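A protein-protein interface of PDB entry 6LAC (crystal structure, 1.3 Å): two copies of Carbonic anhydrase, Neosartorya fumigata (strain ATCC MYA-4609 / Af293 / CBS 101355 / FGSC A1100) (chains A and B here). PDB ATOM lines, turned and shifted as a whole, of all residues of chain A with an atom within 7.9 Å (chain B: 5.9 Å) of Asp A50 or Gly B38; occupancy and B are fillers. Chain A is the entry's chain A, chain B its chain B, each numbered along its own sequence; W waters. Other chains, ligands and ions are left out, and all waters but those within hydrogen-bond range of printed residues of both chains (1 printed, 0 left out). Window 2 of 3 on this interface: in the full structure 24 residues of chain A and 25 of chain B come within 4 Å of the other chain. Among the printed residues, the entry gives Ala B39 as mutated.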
ATOM      1  N   ARG A  22      27.595 -10.180 -17.485  1.00  0.00           N
ATOM      2  CA  ARG A  22      26.163  -9.925 -17.216  1.00  0.00           C
ATOM      3  C   ARG A  22      26.025  -8.706 -16.291  1.00  0.00           C
ATOM      4  O   ARG A  22      25.431  -8.861 -15.212  1.00  0.00           O
ATOM      5  CB  ARG A  22      25.439 -11.141 -16.634  1.00  0.00           C
ATOM      6  CG  ARG A  22      23.936 -11.124 -16.844  1.00  0.00           C
ATOM      7  CD  ARG A  22      23.095 -11.947 -15.914  1.00  0.00           C
ATOM      8  NE  ARG A  22      21.724 -11.977 -16.378  1.00  0.00           N
ATOM      9  CZ  ARG A  22      20.629 -11.932 -15.604  1.00  0.00           C
ATOM     10  NH1 ARG A  22      20.728 -11.838 -14.289  1.00  0.00           N
ATOM     11  NH2 ARG A  22      19.432 -11.916 -16.157  1.00  0.00           N
ATOM     12  N   PRO A  25      20.636  -7.471 -17.167  1.00  0.00           N
ATOM     13  CA  PRO A  25      19.831  -8.592 -17.636  1.00  0.00           C
ATOM     14  C   PRO A  25      19.379  -8.391 -19.086  1.00  0.00           C
ATOM     15  O   PRO A  25      19.466  -7.273 -19.609  1.00  0.00           O
ATOM     16  CB  PRO A  25      18.623  -8.606 -16.690  1.00  0.00           C
ATOM     17  CG  PRO A  25      18.492  -7.165 -16.248  1.00  0.00           C
ATOM     18  CD  PRO A  25      19.911  -6.636 -16.182  1.00  0.00           C
ATOM     19  N   GLY A  26      18.953  -9.499 -19.693  1.00  0.00           N
ATOM     20  CA  GLY A  26      18.173  -9.569 -20.941  1.00  0.00           C
ATOM     21  C   GLY A  26      19.003  -9.476 -22.213  1.00  0.00           C
ATOM     22  O   GLY A  26      18.396  -9.257 -23.248  1.00  0.00           O
ATOM     23  N   GLN A  27      20.335  -9.531 -22.153  1.00  0.00           N
ATOM     24  CA  GLN A  27      21.205  -9.460 -23.361  1.00  0.00           C
ATOM     25  C   GLN A  27      21.605 -10.888 -23.710  1.00  0.00           C
ATOM     26  O   GLN A  27      21.279 -11.786 -22.929  1.00  0.00           O
ATOM     27  CB  GLN A  27      22.440  -8.594 -23.117  1.00  0.00           C
ATOM     28  CG  GLN A  27      22.124  -7.287 -22.388  1.00  0.00           C
ATOM     29  CD  GLN A  27      21.089  -6.463 -23.109  1.00  0.00           C
ATOM     30  OE1 GLN A  27      20.028  -6.134 -22.554  1.00  0.00           O
ATOM     31  NE2 GLN A  27      21.356  -6.194 -24.377  1.00  0.00           N
ATOM     32  N   GLN A  28      22.122 -11.104 -24.901  1.00  0.00           N
ATOM     33  CA  GLN A  28      22.665 -12.431 -25.252  1.00  0.00           C
ATOM     34  C   GLN A  28      24.169 -12.391 -25.148  1.00  0.00           C
ATOM     35  O   GLN A  28      24.809 -11.409 -25.466  1.00  0.00           O
ATOM     36  CB  GLN A  28      22.205 -12.854 -26.624  1.00  0.00           C
ATOM     37  CG  GLN A  28      20.831 -13.505 -26.579  1.00  0.00           C
ATOM     38  CD  GLN A  28      20.425 -13.848 -27.981  1.00  0.00           C
ATOM     39  OE1 GLN A  28      20.260 -12.946 -28.806  1.00  0.00           O
ATOM     40  NE2 GLN A  28      20.381 -15.133 -28.283  1.00  0.00           N
ATOM     41  N   VAL A  29      24.730 -13.519 -24.712  1.00  0.00           N
ATOM     42  CA  VAL A  29      26.191 -13.708 -24.592  1.00  0.00           C
ATOM     43  C   VAL A  29      26.574 -14.885 -25.479  1.00  0.00           C
ATOM     44  O   VAL A  29      25.910 -15.950 -25.384  1.00  0.00           O
ATOM     45  CB  VAL A  29      26.579 -13.953 -23.123  1.00  0.00           C
ATOM     46  CG1 VAL A  29      28.050 -14.260 -23.001  1.00  0.00           C
ATOM     47  CG2 VAL A  29      26.122 -12.784 -22.224  1.00  0.00           C
ATOM     48  N   LEU A  47      24.300 -16.927 -16.084  1.00  0.00           N
ATOM     49  CA  LEU A  47      23.326 -16.506 -17.099  1.00  0.00           C
ATOM     50  C   LEU A  47      22.108 -17.400 -17.052  1.00  0.00           C
ATOM     51  O   LEU A  47      22.236 -18.624 -17.031  1.00  0.00           O
ATOM     52  CB  LEU A  47      23.962 -16.616 -18.493  1.00  0.00           C
ATOM     53  CG  LEU A  47      25.087 -15.637 -18.826  1.00  0.00           C
ATOM     54  CD1 LEU A  47      25.826 -16.037 -20.100  1.00  0.00           C
ATOM     55  CD2 LEU A  47      24.534 -14.235 -18.947  1.00  0.00           C
ATOM     56  N   PRO A  48      20.905 -16.853 -17.195  1.00  0.00           N
ATOM     57  CA  PRO A  48      19.750 -17.676 -17.504  1.00  0.00           C
ATOM     58  C   PRO A  48      19.885 -18.281 -18.906  1.00  0.00           C
ATOM     59  O   PRO A  48      20.585 -17.702 -19.722  1.00  0.00           O
ATOM     60  CB  PRO A  48      18.556 -16.725 -17.444  1.00  0.00           C
ATOM     61  CG  PRO A  48      19.156 -15.373 -17.645  1.00  0.00           C
ATOM     62  CD  PRO A  48      20.610 -15.417 -17.219  1.00  0.00           C
ATOM     63  N   ALA A  49      19.254 -19.417 -19.148  1.00  0.00           N
ATOM     64  CA  ALA A  49      19.390 -20.166 -20.419  1.00  0.00           C
ATOM     65  C   ALA A  49      19.064 -19.274 -21.603  1.00  0.00           C
ATOM     66  O   ALA A  49      19.677 -19.431 -22.682  1.00  0.00           O
ATOM     67  CB  ALA A  49      18.506 -21.385 -20.366  1.00  0.00           C
ATOM     68  N   ASP A  50      18.074 -18.387 -21.470  1.00  0.00           N
ATOM     69  CA  ASP A  50      17.616 -17.605 -22.630  1.00  0.00           C
ATOM     70  C   ASP A  50      18.613 -16.478 -22.977  1.00  0.00           C
ATOM     71  O   ASP A  50      18.435 -15.897 -24.054  1.00  0.00           O
ATOM     72  CB  ASP A  50      16.187 -17.063 -22.425  1.00  0.00           C
ATOM     73  CG  ASP A  50      15.972 -16.089 -21.287  1.00  0.00           C
ATOM     74  OD1 ASP A  50      16.933 -15.682 -20.614  1.00  0.00           O
ATOM     75  OD2 ASP A  50      14.778 -15.757 -21.056  1.00  0.00           O
ATOM     76  N   GLU A  51      19.632 -16.246 -22.164  1.00  0.00           N
ATOM     77  CA  GLU A  51      20.654 -15.228 -22.471  1.00  0.00           C
ATOM     78  C   GLU A  51      21.883 -15.886 -23.106  1.00  0.00           C
ATOM     79  O   GLU A  51      22.887 -15.225 -23.340  1.00  0.00           O
ATOM     80  CB  GLU A  51      21.034 -14.462 -21.205  1.00  0.00           C
ATOM     81  CG  GLU A  51      19.877 -13.592 -20.712  1.00  0.00           C
ATOM     82  CD  GLU A  51      20.225 -12.726 -19.517  1.00  0.00           C
ATOM     83  OE1 GLU A  51      21.393 -12.565 -19.126  1.00  0.00           O
ATOM     84  OE2 GLU A  51      19.222 -12.215 -18.920  1.00  0.00           O
ATOM     85  N   ILE A  52      21.879 -17.197 -23.258  1.00  0.00           N
ATOM     86  CA  ILE A  52      23.063 -17.923 -23.769  1.00  0.00           C
ATOM     87  C   ILE A  52      22.855 -18.232 -25.257  1.00  0.00           C
ATOM     88  O   ILE A  52      21.868 -18.850 -25.614  1.00  0.00           O
ATOM     89  CB  ILE A  52      23.353 -19.190 -22.948  1.00  0.00           C
ATOM     90  CG1 ILE A  52      23.549 -18.881 -21.443  1.00  0.00           C
ATOM     91  CG2 ILE A  52      24.565 -19.946 -23.522  1.00  0.00           C
ATOM     92  CD1 ILE A  52      23.727 -20.126 -20.547  1.00  0.00           C
ATOM     93  N   PHE A  53      23.803 -17.827 -26.073  1.00  0.00           N
ATOM     94  CA  PHE A  53      23.894 -18.222 -27.479  1.00  0.00           C
ATOM     95  C   PHE A  53      25.149 -19.082 -27.515  1.00  0.00           C
ATOM     96  O   PHE A  53      26.259 -18.574 -27.372  1.00  0.00           O
ATOM     97  CB  PHE A  53      23.943 -16.962 -28.351  1.00  0.00           C
ATOM     98  CG  PHE A  53      24.011 -17.287 -29.811  1.00  0.00           C
ATOM     99  CD1 PHE A  53      22.876 -17.694 -30.476  1.00  0.00           C
ATOM    100  CD2 PHE A  53      25.200 -17.172 -30.504  1.00  0.00           C
ATOM    101  CE1 PHE A  53      22.963 -18.029 -31.814  1.00  0.00           C
ATOM    102  CE2 PHE A  53      25.271 -17.541 -31.849  1.00  0.00           C
ATOM    103  CZ  PHE A  53      24.146 -17.962 -32.482  1.00  0.00           C
ATOM    104  N   GLU A  54      24.963 -20.395 -27.629  1.00  0.00           N
ATOM    105  CA  GLU A  54      26.025 -21.358 -27.280  1.00  0.00           C
ATOM    106  C   GLU A  54      26.664 -21.918 -28.542  1.00  0.00           C
ATOM    107  O   GLU A  54      25.922 -22.539 -29.352  1.00  0.00           O
ATOM    108  CB  GLU A  54      25.394 -22.423 -26.403  1.00  0.00           C
ATOM    109  CG  GLU A  54      26.376 -23.451 -25.887  1.00  0.00           C
ATOM    110  CD  GLU A  54      25.755 -24.502 -24.967  1.00  0.00           C
ATOM    111  OE1 GLU A  54      24.523 -24.610 -24.970  1.00  0.00           O
ATOM    112  OE2 GLU A  54      26.525 -25.247 -24.327  1.00  0.00           O
ATOM    113  N   CYS B  34      21.262 -26.648 -31.774  1.00  0.00           N
ATOM    114  CA  CYS B  34      21.322 -25.268 -32.250  1.00  0.00           C
ATOM    115  C   CYS B  34      21.743 -24.291 -31.157  1.00  0.00           C
ATOM    116  O   CYS B  34      21.304 -24.326 -30.028  1.00  0.00           O
ATOM    117  CB  CYS B  34      20.002 -24.815 -32.784  1.00  0.00           C
ATOM    118  SG  CYS B  34      20.004 -23.140 -33.486  1.00  0.00           S
ATOM    119  N   SER B  35      22.616 -23.359 -31.593  1.00  0.00           N
ATOM    120  CA  SER B  35      23.139 -22.272 -30.728  1.00  0.00           C
ATOM    121  C   SER B  35      22.052 -21.440 -30.060  1.00  0.00           C
ATOM    122  O   SER B  35      22.366 -20.924 -28.979  1.00  0.00           O
ATOM    123  CB  SER B  35      24.076 -21.401 -31.476  1.00  0.00           C
ATOM    124  OG  SER B  35      25.179 -22.183 -31.958  1.00  0.00           O
ATOM    125  N   ASP B  36      20.875 -21.252 -30.657  1.00  0.00           N
ATOM    126  CA  ASP B  36      19.860 -20.390 -29.985  1.00  0.00           C
ATOM    127  C   ASP B  36      18.821 -21.207 -29.266  1.00  0.00           C
ATOM    128  O   ASP B  36      17.770 -20.646 -28.863  1.00  0.00           O
ATOM    129  CB  ASP B  36      19.308 -19.336 -30.957  1.00  0.00           C
ATOM    130  CG  ASP B  36      18.409 -19.880 -32.045  1.00  0.00           C
ATOM    131  OD1 ASP B  36      17.970 -21.056 -31.932  1.00  0.00           O
ATOM    132  OD2 ASP B  36      18.051 -19.157 -32.993  1.00  0.00           O
ATOM    133  N   SER B  37      19.047 -22.493 -28.998  1.00  0.00           N
ATOM    134  CA  SER B  37      18.027 -23.293 -28.295  1.00  0.00           C
ATOM    135  C   SER B  37      17.606 -22.631 -26.987  1.00  0.00           C
ATOM    136  O   SER B  37      16.415 -22.556 -26.703  1.00  0.00           O
ATOM    137  CB  SER B  37      18.564 -24.699 -28.136  1.00  0.00           C
ATOM    138  OG  SER B  37      17.571 -25.558 -27.556  1.00  0.00           O
ATOM    139  N   GLY B  38      18.522 -22.112 -26.196  1.00  0.00           N
ATOM    140  CA  GLY B  38      18.197 -21.101 -25.176  1.00  0.00           C
ATOM    141  C   GLY B  38      17.334 -21.638 -24.069  1.00  0.00           C
ATOM    142  O   GLY B  38      16.586 -20.789 -23.500  1.00  0.00           O
ATOM    143  N   ALA B  39      17.391 -22.923 -23.717  1.00  0.00           N
ATOM    144  CA  ALA B  39      16.469 -23.508 -22.720  1.00  0.00           C
ATOM    145  C   ALA B  39      17.095 -24.777 -22.132  1.00  0.00           C
ATOM    146  O   ALA B  39      18.306 -24.755 -21.756  1.00  0.00           O
ATOM    147  CB  ALA B  39      15.152 -23.758 -23.374  1.00  0.00           C
ATOM    148  N   ASP B  40      16.309 -25.839 -21.941  1.00  0.00           N
ATOM    149  CA  ASP B  40      16.734 -27.045 -21.209  1.00  0.00           C
ATOM    150  C   ASP B  40      16.698 -28.244 -22.142  1.00  0.00           C
ATOM    151  O   ASP B  40      16.316 -29.354 -21.733  1.00  0.00           O
ATOM    152  CB  ASP B  40      15.841 -27.276 -19.978  1.00  0.00           C
ATOM    153  CG  ASP B  40      15.903 -26.152 -18.967  1.00  0.00           C
ATOM    154  OD1 ASP B  40      14.839 -25.807 -18.448  1.00  0.00           O
ATOM    155  OD2 ASP B  40      17.016 -25.618 -18.702  1.00  0.00           O
ATOM    156  N   HIS B  89      14.766 -27.396 -32.572  1.00  0.00           N
ATOM    157  CA  HIS B  89      13.929 -26.892 -31.468  1.00  0.00           C
ATOM    158  C   HIS B  89      12.925 -25.866 -31.952  1.00  0.00           C
ATOM    159  O   HIS B  89      13.255 -24.995 -32.730  1.00  0.00           O
ATOM    160  CB  HIS B  89      14.786 -26.354 -30.338  1.00  0.00           C
ATOM    161  CG  HIS B  89      15.523 -25.133 -30.748  1.00  0.00           C
ATOM    162  ND1 HIS B  89      15.173 -23.861 -30.336  1.00  0.00           N
ATOM    163  CD2 HIS B  89      16.503 -24.942 -31.669  1.00  0.00           C
ATOM    164  CE1 HIS B  89      15.944 -22.986 -30.911  1.00  0.00           C
ATOM    165  NE2 HIS B  89      16.792 -23.620 -31.715  1.00  0.00           N
ATOM    166  N   LYS B 170      10.492 -26.389 -25.855  1.00  0.00           N
ATOM    167  CA  LYS B 170      10.762 -25.839 -24.506  1.00  0.00           C
ATOM    168  C   LYS B 170       9.461 -25.490 -23.770  1.00  0.00           C
ATOM    169  O   LYS B 170       9.483 -25.575 -22.528  1.00  0.00           O
ATOM    170  CB  LYS B 170      11.701 -24.639 -24.625  1.00  0.00           C
ATOM    171  CG  LYS B 170      11.110 -23.452 -25.340  1.00  0.00           C
ATOM    172  CD  LYS B 170      12.083 -22.264 -25.427  1.00  0.00           C
ATOM    173  CE  LYS B 170      11.609 -21.107 -26.267  1.00  0.00           C
ATOM    174  NZ  LYS B 170      11.666 -21.371 -27.712  1.00  0.00           N
HETATM  175  O   HOH W   1      21.330 -21.429 -26.482  1.00  0.00           O
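Printed residues of chain A that touch a printed residue of chain B: Ala A49, Asp A50, Ile A52, Phe A53 and Glu A54.
Hydrophobic or aromatic side chains of chain A that line the printed part of chain B: Ala A49 and Phe A53.
Printed residues of chain B that touch a printed residue of chain A: Ser B35, Asp B36, Gly B38 and Ala B39.
Among the printed residues, no Asp or Glu carboxylate lies within 4 Å of a Lys or Arg side-chain nitrogen of the other chain.
Water W1 lies within hydrogen-bond range of O of Ser B35 (2.8 Å), O of Ile A52 (2.8 Å) and N of Gly B38 (2.9 Å).
Among the printed residues, pairs that only touch across the chains: Phe A53 with Ser B35 (3.4 Å), Ala A49 with Ala B39 (3.7 Å), Phe A53 with Asp B36 (3.96 Å) and Ile A52 with Ser B35 (3.98 Å).
Printed residues of chain B within 4 Å of Ala A49: Gly B38 and Ala B39.
Of chain B, only Gly B38 comes within 4 Å of Asp A50.
Of the printed residues of chain B, Phe A53 touches Ser B35 (3.4 Å) and Asp B36 (3.96 Å).
Cys B34 touches none of the printed residues of chain A.
Of the printed residues of chain A, Asp B36 touches Phe A53.
Printed residues of chain A within 4 Å of Gly B38: Ala A49 and Asp A50.
The nearest residue of chain B that does not touch Asp A50 is Ala B39 (5.1 Å).
The backbone carbonyl oxygen of Val A29 sits at hydrogen-bond distance from the backbone NH of Phe A53, at 2.9 Å.
No position is printed for both chains.
Of the 7 pairs that touch across the chains among the printed residues, none has its exchanged pair printed and touching as well.
The backbone carbonyl oxygen of Gly B38 sits close to the backbone NH of Asp A50 (3.5 Å).
The side-chain hydroxyl (OG) of Ser B35 is in hydrogen-bond range of the backbone carbonyl oxygen (O) of Glu A54, 2.7 Å away.
The backbone carbonyl oxygen (O) of Ala A49 lies close to the backbone carbonyl oxygen (O) of Gly B38 (3.5 Å).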
